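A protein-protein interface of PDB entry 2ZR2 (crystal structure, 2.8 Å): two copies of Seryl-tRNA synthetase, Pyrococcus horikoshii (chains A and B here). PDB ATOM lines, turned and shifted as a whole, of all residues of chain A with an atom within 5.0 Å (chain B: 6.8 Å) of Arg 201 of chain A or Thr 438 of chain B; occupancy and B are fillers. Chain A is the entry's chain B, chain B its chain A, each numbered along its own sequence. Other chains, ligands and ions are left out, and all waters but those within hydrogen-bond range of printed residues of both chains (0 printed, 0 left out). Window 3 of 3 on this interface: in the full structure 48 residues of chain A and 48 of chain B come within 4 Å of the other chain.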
ATOM      1  N   LEU A 197      21.273 -24.345   6.714  1.00  0.00           N
ATOM      2  CA  LEU A 197      20.864 -23.176   7.489  1.00  0.00           C
ATOM      3  C   LEU A 197      19.416 -23.287   7.957  1.00  0.00           C
ATOM      4  O   LEU A 197      19.085 -22.912   9.084  1.00  0.00           O
ATOM      5  CB  LEU A 197      21.066 -21.900   6.678  1.00  0.00           C
ATOM      6  CG  LEU A 197      22.513 -21.748   6.183  1.00  0.00           C
ATOM      7  CD1 LEU A 197      22.618 -20.471   5.390  1.00  0.00           C
ATOM      8  CD2 LEU A 197      23.514 -21.731   7.345  1.00  0.00           C
ATOM      9  N   ALA A 198      18.555 -23.819   7.095  1.00  0.00           N
ATOM     10  CA  ALA A 198      17.147 -23.976   7.420  1.00  0.00           C
ATOM     11  C   ALA A 198      16.933 -24.871   8.653  1.00  0.00           C
ATOM     12  O   ALA A 198      15.988 -24.669   9.419  1.00  0.00           O
ATOM     13  CB  ALA A 198      16.406 -24.531   6.209  1.00  0.00           C
ATOM     14  N   LEU A 199      17.806 -25.854   8.860  1.00  0.00           N
ATOM     15  CA  LEU A 199      17.671 -26.719  10.027  1.00  0.00           C
ATOM     16  C   LEU A 199      18.043 -25.969  11.307  1.00  0.00           C
ATOM     17  O   LEU A 199      17.416 -26.156  12.354  1.00  0.00           O
ATOM     18  CB  LEU A 199      18.531 -27.975   9.868  1.00  0.00           C
ATOM     19  CG  LEU A 199      17.942 -28.972   8.861  1.00  0.00           C
ATOM     20  CD1 LEU A 199      19.013 -29.940   8.416  1.00  0.00           C
ATOM     21  CD2 LEU A 199      16.755 -29.698   9.486  1.00  0.00           C
ATOM     22  N   ILE A 200      19.062 -25.120  11.223  1.00  0.00           N
ATOM     23  CA  ILE A 200      19.473 -24.340  12.374  1.00  0.00           C
ATOM     24  C   ILE A 200      18.321 -23.420  12.755  1.00  0.00           C
ATOM     25  O   ILE A 200      17.912 -23.340  13.919  1.00  0.00           O
ATOM     26  CB  ILE A 200      20.698 -23.464  12.044  1.00  0.00           C
ATOM     27  CG1 ILE A 200      21.955 -24.329  11.979  1.00  0.00           C
ATOM     28  CG2 ILE A 200      20.851 -22.353  13.078  1.00  0.00           C
ATOM     29  CD1 ILE A 200      23.091 -23.661  11.242  1.00  0.00           C
ATOM     30  N   ARG A 201      17.786 -22.723  11.764  1.00  0.00           N
ATOM     31  CA  ARG A 201      16.708 -21.792  12.051  1.00  0.00           C
ATOM     32  C   ARG A 201      15.445 -22.477  12.551  1.00  0.00           C
ATOM     33  O   ARG A 201      14.763 -21.981  13.451  1.00  0.00           O
ATOM     34  CB  ARG A 201      16.411 -20.930  10.835  1.00  0.00           C
ATOM     35  CG  ARG A 201      15.392 -19.864  11.121  1.00  0.00           C
ATOM     36  CD  ARG A 201      15.682 -19.081  12.404  1.00  0.00           C
ATOM     37  NE  ARG A 201      14.595 -18.140  12.639  1.00  0.00           N
ATOM     38  CZ  ARG A 201      14.422 -17.036  11.922  1.00  0.00           C
ATOM     39  NH1 ARG A 201      13.397 -16.227  12.171  1.00  0.00           N
ATOM     40  NH2 ARG A 201      15.306 -16.726  10.975  1.00  0.00           N
ATOM     41  N   PHE A 202      15.135 -23.627  11.984  1.00  0.00           N
ATOM     42  CA  PHE A 202      13.968 -24.356  12.435  1.00  0.00           C
ATOM     43  C   PHE A 202      14.138 -24.710  13.931  1.00  0.00           C
ATOM     44  O   PHE A 202      13.252 -24.449  14.737  1.00  0.00           O
ATOM     45  CB  PHE A 202      13.804 -25.596  11.557  1.00  0.00           C
ATOM     46  CG  PHE A 202      12.830 -26.593  12.080  1.00  0.00           C
ATOM     47  CD1 PHE A 202      11.516 -26.230  12.345  1.00  0.00           C
ATOM     48  CD2 PHE A 202      13.230 -27.920  12.291  1.00  0.00           C
ATOM     49  CE1 PHE A 202      10.608 -27.175  12.810  1.00  0.00           C
ATOM     50  CE2 PHE A 202      12.333 -28.877  12.757  1.00  0.00           C
ATOM     51  CZ  PHE A 202      11.016 -28.508  13.019  1.00  0.00           C
ATOM     52  N   ALA A 203      15.284 -25.271  14.307  1.00  0.00           N
ATOM     53  CA  ALA A 203      15.525 -25.639  15.703  1.00  0.00           C
ATOM     54  C   ALA A 203      15.443 -24.422  16.623  1.00  0.00           C
ATOM     55  O   ALA A 203      14.816 -24.484  17.694  1.00  0.00           O
ATOM     56  CB  ALA A 203      16.885 -26.323  15.847  1.00  0.00           C
ATOM     57  N   LEU A 204      16.087 -23.326  16.210  1.00  0.00           N
ATOM     58  CA  LEU A 204      16.050 -22.088  16.979  1.00  0.00           C
ATOM     59  C   LEU A 204      14.611 -21.641  17.255  1.00  0.00           C
ATOM     60  O   LEU A 204      14.250 -21.363  18.399  1.00  0.00           O
ATOM     61  CB  LEU A 204      16.762 -20.959  16.240  1.00  0.00           C
ATOM     62  CG  LEU A 204      18.175 -20.548  16.651  1.00  0.00           C
ATOM     63  CD1 LEU A 204      18.542 -21.157  17.986  1.00  0.00           C
ATOM     64  CD2 LEU A 204      19.150 -20.992  15.580  1.00  0.00           C
ATOM     65  N   ASP A 205      13.782 -21.574  16.219  1.00  0.00           N
ATOM     66  CA  ASP A 205      12.404 -21.133  16.425  1.00  0.00           C
ATOM     67  C   ASP A 205      11.640 -22.022  17.401  1.00  0.00           C
ATOM     68  O   ASP A 205      10.998 -21.532  18.337  1.00  0.00           O
ATOM     69  CB  ASP A 205      11.637 -21.051  15.097  1.00  0.00           C
ATOM     70  CG  ASP A 205      12.225 -20.015  14.140  1.00  0.00           C
ATOM     71  OD1 ASP A 205      12.983 -19.121  14.602  1.00  0.00           O
ATOM     72  OD2 ASP A 205      11.918 -20.093  12.922  1.00  0.00           O
ATOM     73  N   TYR A 437      11.306 -22.478   5.213  1.00  0.00           N
ATOM     74  CA  TYR A 437      12.711 -22.092   5.363  1.00  0.00           C
ATOM     75  C   TYR A 437      13.565 -22.356   4.142  1.00  0.00           C
ATOM     76  O   TYR A 437      14.534 -21.639   3.901  1.00  0.00           O
ATOM     77  CB  TYR A 437      13.383 -22.796   6.549  1.00  0.00           C
ATOM     78  CG  TYR A 437      12.705 -22.630   7.889  1.00  0.00           C
ATOM     79  CD1 TYR A 437      11.812 -23.593   8.365  1.00  0.00           C
ATOM     80  CD2 TYR A 437      12.980 -21.527   8.706  1.00  0.00           C
ATOM     81  CE1 TYR A 437      11.214 -23.466   9.626  1.00  0.00           C
ATOM     82  CE2 TYR A 437      12.380 -21.391   9.977  1.00  0.00           C
ATOM     83  CZ  TYR A 437      11.507 -22.365  10.427  1.00  0.00           C
ATOM     84  OH  TYR A 437      10.960 -22.271  11.691  1.00  0.00           O
ATOM     85  N   GLU B 191      17.020 -11.404  19.886  1.00  0.00           N
ATOM     86  CA  GLU B 191      16.789 -10.876  18.551  1.00  0.00           C
ATOM     87  C   GLU B 191      18.062 -10.706  17.755  1.00  0.00           C
ATOM     88  O   GLU B 191      18.064 -10.920  16.539  1.00  0.00           O
ATOM     89  CB  GLU B 191      16.069  -9.545  18.636  1.00  0.00           C
ATOM     90  CG  GLU B 191      16.159  -8.965  20.029  1.00  0.00           C
ATOM     91  CD  GLU B 191      15.045  -9.477  20.884  1.00  0.00           C
ATOM     92  OE1 GLU B 191      15.090  -9.344  22.131  1.00  0.00           O
ATOM     93  OE2 GLU B 191      14.103 -10.000  20.275  1.00  0.00           O
ATOM     94  N   ILE B 194      18.880 -13.776  15.840  1.00  0.00           N
ATOM     95  CA  ILE B 194      18.010 -13.990  14.687  1.00  0.00           C
ATOM     96  C   ILE B 194      18.403 -13.046  13.573  1.00  0.00           C
ATOM     97  O   ILE B 194      18.364 -13.407  12.400  1.00  0.00           O
ATOM     98  CB  ILE B 194      16.536 -13.730  15.011  1.00  0.00           C
ATOM     99  CG1 ILE B 194      16.050 -14.735  16.059  1.00  0.00           C
ATOM    100  CG2 ILE B 194      15.708 -13.825  13.745  1.00  0.00           C
ATOM    101  CD1 ILE B 194      16.297 -16.181  15.703  1.00  0.00           C
ATOM    102  N   LEU B 195      18.768 -11.826  13.953  1.00  0.00           N
ATOM    103  CA  LEU B 195      19.184 -10.828  12.984  1.00  0.00           C
ATOM    104  C   LEU B 195      20.463 -11.288  12.279  1.00  0.00           C
ATOM    105  O   LEU B 195      20.624 -11.092  11.064  1.00  0.00           O
ATOM    106  CB  LEU B 195      19.421  -9.483  13.677  1.00  0.00           C
ATOM    107  CG  LEU B 195      19.941  -8.348  12.785  1.00  0.00           C
ATOM    108  CD1 LEU B 195      18.931  -8.016  11.677  1.00  0.00           C
ATOM    109  CD2 LEU B 195      20.200  -7.139  13.641  1.00  0.00           C
ATOM    110  N   ASP B 196      21.375 -11.889  13.047  1.00  0.00           N
ATOM    111  CA  ASP B 196      22.623 -12.383  12.483  1.00  0.00           C
ATOM    112  C   ASP B 196      22.296 -13.425  11.417  1.00  0.00           C
ATOM    113  O   ASP B 196      22.703 -13.278  10.263  1.00  0.00           O
ATOM    114  CB  ASP B 196      23.500 -13.016  13.567  1.00  0.00           C
ATOM    115  CG  ASP B 196      24.856 -13.466  13.040  1.00  0.00           C
ATOM    116  OD1 ASP B 196      25.874 -12.949  13.518  1.00  0.00           O
ATOM    117  OD2 ASP B 196      24.918 -14.332  12.149  1.00  0.00           O
ATOM    118  N   LEU B 197      21.552 -14.464  11.791  1.00  0.00           N
ATOM    119  CA  LEU B 197      21.201 -15.498  10.824  1.00  0.00           C
ATOM    120  C   LEU B 197      20.454 -14.921   9.649  1.00  0.00           C
ATOM    121  O   LEU B 197      20.690 -15.313   8.505  1.00  0.00           O
ATOM    122  CB  LEU B 197      20.331 -16.580  11.445  1.00  0.00           C
ATOM    123  CG  LEU B 197      20.924 -17.384  12.600  1.00  0.00           C
ATOM    124  CD1 LEU B 197      19.958 -18.530  12.925  1.00  0.00           C
ATOM    125  CD2 LEU B 197      22.331 -17.915  12.244  1.00  0.00           C
ATOM    126  N   ALA B 198      19.550 -13.992   9.940  1.00  0.00           N
ATOM    127  CA  ALA B 198      18.743 -13.358   8.899  1.00  0.00           C
ATOM    128  C   ALA B 198      19.625 -12.699   7.856  1.00  0.00           C
ATOM    129  O   ALA B 198      19.389 -12.845   6.660  1.00  0.00           O
ATOM    130  CB  ALA B 198      17.786 -12.327   9.513  1.00  0.00           C
ATOM    131  N   LEU B 199      20.650 -11.989   8.312  1.00  0.00           N
ATOM    132  CA  LEU B 199      21.556 -11.302   7.404  1.00  0.00           C
ATOM    133  C   LEU B 199      22.305 -12.272   6.506  1.00  0.00           C
ATOM    134  O   LEU B 199      22.579 -11.960   5.358  1.00  0.00           O
ATOM    135  CB  LEU B 199      22.526 -10.422   8.206  1.00  0.00           C
ATOM    136  CG  LEU B 199      21.891  -9.139   8.778  1.00  0.00           C
ATOM    137  CD1 LEU B 199      22.724  -8.544   9.898  1.00  0.00           C
ATOM    138  CD2 LEU B 199      21.719  -8.137   7.646  1.00  0.00           C
ATOM    139  N   ARG B 201      21.133 -15.325   5.482  1.00  0.00           N
ATOM    140  CA  ARG B 201      20.180 -15.789   4.472  1.00  0.00           C
ATOM    141  C   ARG B 201      19.899 -14.734   3.404  1.00  0.00           C
ATOM    142  O   ARG B 201      19.933 -15.029   2.209  1.00  0.00           O
ATOM    143  CB  ARG B 201      18.859 -16.230   5.104  1.00  0.00           C
ATOM    144  CG  ARG B 201      18.789 -17.719   5.421  1.00  0.00           C
ATOM    145  CD  ARG B 201      19.386 -18.572   4.296  1.00  0.00           C
ATOM    146  NE  ARG B 201      18.602 -18.612   3.059  1.00  0.00           N
ATOM    147  CZ  ARG B 201      17.499 -19.340   2.888  1.00  0.00           C
ATOM    148  NH1 ARG B 201      16.868 -19.312   1.727  1.00  0.00           N
ATOM    149  NH2 ARG B 201      17.021 -20.090   3.877  1.00  0.00           N
ATOM    150  N   ILE B 430      13.838  -2.670  12.208  1.00  0.00           N
ATOM    151  CA  ILE B 430      14.532  -3.553  11.280  1.00  0.00           C
ATOM    152  C   ILE B 430      14.131  -3.223   9.854  1.00  0.00           C
ATOM    153  O   ILE B 430      12.960  -3.105   9.565  1.00  0.00           O
ATOM    154  CB  ILE B 430      14.241  -5.064  11.564  1.00  0.00           C
ATOM    155  CG1 ILE B 430      15.186  -5.587  12.644  1.00  0.00           C
ATOM    156  CG2 ILE B 430      14.519  -5.913  10.322  1.00  0.00           C
ATOM    157  CD1 ILE B 430      14.999  -4.946  13.974  1.00  0.00           C
ATOM    158  N   PRO B 431      15.113  -3.068   8.943  1.00  0.00           N
ATOM    159  CA  PRO B 431      14.828  -2.755   7.534  1.00  0.00           C
ATOM    160  C   PRO B 431      13.765  -3.708   7.016  1.00  0.00           C
ATOM    161  O   PRO B 431      13.897  -4.916   7.189  1.00  0.00           O
ATOM    162  CB  PRO B 431      16.166  -3.001   6.845  1.00  0.00           C
ATOM    163  CG  PRO B 431      17.167  -2.702   7.930  1.00  0.00           C
ATOM    164  CD  PRO B 431      16.555  -3.319   9.152  1.00  0.00           C
ATOM    165  N   LEU B 434      14.322  -7.342   5.642  1.00  0.00           N
ATOM    166  CA  LEU B 434      14.680  -8.479   6.512  1.00  0.00           C
ATOM    167  C   LEU B 434      13.521  -9.093   7.279  1.00  0.00           C
ATOM    168  O   LEU B 434      13.690 -10.120   7.940  1.00  0.00           O
ATOM    169  CB  LEU B 434      15.738  -8.075   7.538  1.00  0.00           C
ATOM    170  CG  LEU B 434      17.064  -7.673   6.926  1.00  0.00           C
ATOM    171  CD1 LEU B 434      18.041  -7.253   8.020  1.00  0.00           C
ATOM    172  CD2 LEU B 434      17.577  -8.849   6.111  1.00  0.00           C
ATOM    173  N   TRP B 435      12.354  -8.461   7.208  1.00  0.00           N
ATOM    174  CA  TRP B 435      11.193  -8.959   7.927  1.00  0.00           C
ATOM    175  C   TRP B 435      10.903 -10.424   7.603  1.00  0.00           C
ATOM    176  O   TRP B 435      10.704 -11.228   8.515  1.00  0.00           O
ATOM    177  CB  TRP B 435       9.967  -8.086   7.640  1.00  0.00           C
ATOM    178  CG  TRP B 435      10.075  -6.713   8.215  1.00  0.00           C
ATOM    179  CD1 TRP B 435      11.049  -6.246   9.056  1.00  0.00           C
ATOM    180  CD2 TRP B 435       9.180  -5.619   8.001  1.00  0.00           C
ATOM    181  NE1 TRP B 435      10.819  -4.929   9.374  1.00  0.00           N
ATOM    182  CE2 TRP B 435       9.677  -4.520   8.740  1.00  0.00           C
ATOM    183  CE3 TRP B 435       8.006  -5.458   7.258  1.00  0.00           C
ATOM    184  CZ2 TRP B 435       9.038  -3.281   8.756  1.00  0.00           C
ATOM    185  CZ3 TRP B 435       7.374  -4.228   7.273  1.00  0.00           C
ATOM    186  CH2 TRP B 435       7.891  -3.154   8.017  1.00  0.00           C
ATOM    187  N   LYS B 436      10.905 -10.783   6.320  1.00  0.00           N
ATOM    188  CA  LYS B 436      10.634 -12.166   5.963  1.00  0.00           C
ATOM    189  C   LYS B 436      11.603 -13.103   6.661  1.00  0.00           C
ATOM    190  O   LYS B 436      11.293 -14.283   6.847  1.00  0.00           O
ATOM    191  CB  LYS B 436      10.673 -12.388   4.439  1.00  0.00           C
ATOM    192  CG  LYS B 436      11.964 -12.031   3.736  1.00  0.00           C
ATOM    193  CD  LYS B 436      11.808 -12.243   2.233  1.00  0.00           C
ATOM    194  CE  LYS B 436      12.935 -11.601   1.417  1.00  0.00           C
ATOM    195  NZ  LYS B 436      12.782 -10.115   1.220  1.00  0.00           N
ATOM    196  N   TYR B 437      12.757 -12.583   7.086  1.00  0.00           N
ATOM    197  CA  TYR B 437      13.735 -13.428   7.768  1.00  0.00           C
ATOM    198  C   TYR B 437      13.710 -13.349   9.277  1.00  0.00           C
ATOM    199  O   TYR B 437      13.980 -14.342   9.945  1.00  0.00           O
ATOM    200  CB  TYR B 437      15.158 -13.120   7.325  1.00  0.00           C
ATOM    201  CG  TYR B 437      15.382 -13.197   5.846  1.00  0.00           C
ATOM    202  CD1 TYR B 437      15.498 -12.033   5.085  1.00  0.00           C
ATOM    203  CD2 TYR B 437      15.504 -14.430   5.199  1.00  0.00           C
ATOM    204  CE1 TYR B 437      15.731 -12.091   3.712  1.00  0.00           C
ATOM    205  CE2 TYR B 437      15.742 -14.497   3.822  1.00  0.00           C
ATOM    206  CZ  TYR B 437      15.854 -13.322   3.086  1.00  0.00           C
ATOM    207  OH  TYR B 437      16.087 -13.361   1.731  1.00  0.00           O
ATOM    208  N   THR B 438      13.396 -12.185   9.829  1.00  0.00           N
ATOM    209  CA  THR B 438      13.404 -12.049  11.284  1.00  0.00           C
ATOM    210  C   THR B 438      12.099 -12.347  11.979  1.00  0.00           C
ATOM    211  O   THR B 438      12.079 -12.955  13.043  1.00  0.00           O
ATOM    212  CB  THR B 438      13.821 -10.647  11.697  1.00  0.00           C
ATOM    213  OG1 THR B 438      12.919  -9.694  11.115  1.00  0.00           O
ATOM    214  CG2 THR B 438      15.247 -10.377  11.238  1.00  0.00           C
ATOM    215  N   GLY B 439      11.003 -11.918  11.368  1.00  0.00           N
ATOM    216  CA  GLY B 439       9.708 -12.122  11.973  1.00  0.00           C
ATOM    217  C   GLY B 439       9.352 -10.787  12.577  1.00  0.00           C
ATOM    218  O   GLY B 439       8.435 -10.112  12.117  1.00  0.00           O
ATOM    219  N   PHE B 440      10.101 -10.388  13.593  1.00  0.00           N
ATOM    220  CA  PHE B 440       9.872  -9.117  14.251  1.00  0.00           C
ATOM    221  C   PHE B 440      10.249  -7.964  13.319  1.00  0.00           C
ATOM    222  O   PHE B 440      11.064  -8.144  12.419  1.00  0.00           O
ATOM    223  CB  PHE B 440      10.694  -9.076  15.526  1.00  0.00           C
ATOM    224  CG  PHE B 440      12.144  -9.391  15.319  1.00  0.00           C
ATOM    225  CD1 PHE B 440      13.018  -8.428  14.822  1.00  0.00           C
ATOM    226  CD2 PHE B 440      12.650 -10.649  15.648  1.00  0.00           C
ATOM    227  CE1 PHE B 440      14.377  -8.722  14.663  1.00  0.00           C
ATOM    228  CE2 PHE B 440      14.008 -10.946  15.489  1.00  0.00           C
ATOM    229  CZ  PHE B 440      14.870  -9.986  14.998  1.00  0.00           C
ATOM    230  N   LYS B 441       9.652  -6.787  13.529  1.00  0.00           N
ATOM    231  CA  LYS B 441       9.940  -5.628  12.679  1.00  0.00           C
ATOM    232  C   LYS B 441      10.843  -4.607  13.349  1.00  0.00           C
ATOM    233  O   LYS B 441      11.318  -3.669  12.709  1.00  0.00           O
ATOM    234  CB  LYS B 441       8.653  -4.922  12.250  1.00  0.00           C
ATOM    235  CG  LYS B 441       7.636  -5.791  11.536  1.00  0.00           C
ATOM    236  CD  LYS B 441       6.656  -4.939  10.767  1.00  0.00           C
ATOM    237  CE  LYS B 441       5.418  -5.726  10.367  1.00  0.00           C
ATOM    238  NZ  LYS B 441       4.628  -6.170  11.559  1.00  0.00           N
ATOM    239  N   GLU B 442      11.082  -4.789  14.639  1.00  0.00           N
ATOM    240  CA  GLU B 442      11.935  -3.884  15.391  1.00  0.00           C
ATOM    241  C   GLU B 442      12.331  -4.583  16.675  1.00  0.00           C
ATOM    242  O   GLU B 442      11.725  -5.578  17.054  1.00  0.00           O
ATOM    243  CB  GLU B 442      11.172  -2.619  15.751  1.00  0.00           C
ATOM    244  CG  GLU B 442       9.851  -2.910  16.459  1.00  0.00           C
ATOM    245  CD  GLU B 442       9.210  -1.670  17.051  1.00  0.00           C
ATOM    246  OE1 GLU B 442       9.331  -0.575  16.442  1.00  0.00           O
ATOM    247  OE2 GLU B 442       8.573  -1.799  18.121  1.00  0.00           O
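The guanidinium group of Arg 201 of chain B lies within hydrogen-bond range of the backbone carbonyl oxygen of Tyr 437 of chain A (2.9 Å).
The guanidinium group (NH2) of Arg 201 of chain A lies within hydrogen-bond range of the backbone carbonyl oxygen (O) of Tyr 437 of chain B (2.9 Å).
OD2 of Asp 205 of chain A sits at hydrogen-bond distance from OH of Tyr 437 of chain A, 2.7 Å away.
O of Leu 434 of chain B lies within hydrogen-bond range of OG1 of Thr 438 of chain B (3.3 Å).
The guanidinium group of Arg 201 of chain A is in salt-bridge range of the side-chain carboxylate of Asp 205 of chain A, at 2.7 Å.
OG1 of Thr 438 of chain B lies within hydrogen-bond range of O of Phe 440 of chain B, at 2.7 Å.
Among the printed residues, pairs that only touch across the chains: Arg 201 of chain A with Thr 438 of chain B (3.6 Å), Arg 201 of chain A with Ile 194 of chain B (3.7 Å), Leu 204 of chain A with Leu 197 of chain B (3.7 Å), Leu 197 of chain A with Arg 201 of chain B (3.9 Å) and Ile 200 of chain A with Leu 197 of chain B (3.9 Å).
Printed residues of chain B within 4 Å of Ile 200 of chain A: Leu 197 (3.9 Å).
Arg 201 of chain A touches three residues of chain B.
Printed residues of chain B within 4 Å of Leu 204 of chain A: Leu 197.
Printed residues of chain A within 4 Å of Ile 194 of chain B: Arg 201 (3.7 Å).
Printed residues of chain A within 4 Å of Leu 197 of chain B: Ile 200 (3.9 Å) and Leu 204 (3.7 Å).
Of the printed residues of chain A, Arg 201 of chain B touches Leu 197 (3.9 Å) and Tyr 437 (2.9 Å).
Thr 438 of chain B touches just one residue of chain A: Arg 201.
Lys 441 of chain B touches none of the printed residues of chain A.
The nearest residue of chain B that does not touch Arg 201 of chain A is Leu 197 of chain B (4.3 Å).
Hydrophobic or aromatic side chains of chain A within 4 Å of the printed part of chain B: Leu 197, Ile 200 and Leu 204.
Of the 19 printed residues of chain B, 5 touch a printed residue of chain A.
Among the printed residues, no Asp or Glu carboxylate lies within 4 Å of a Lys or Arg side-chain nitrogen of the other chain.
Leu 197 of chain A touches Arg 201 of chain B, but with the chains exchanged Arg 201 of chain A does not touch Leu 197 of chain B (4.3 Å).
Arg 201 of chain A touches Tyr 437 of chain B, and with the chains exchanged Tyr 437 of chain A touches Arg 201 of chain B.
Of the 7 pairs that touch across the chains among the printed residues, 2 have their exchanged pair printed and touching as well.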
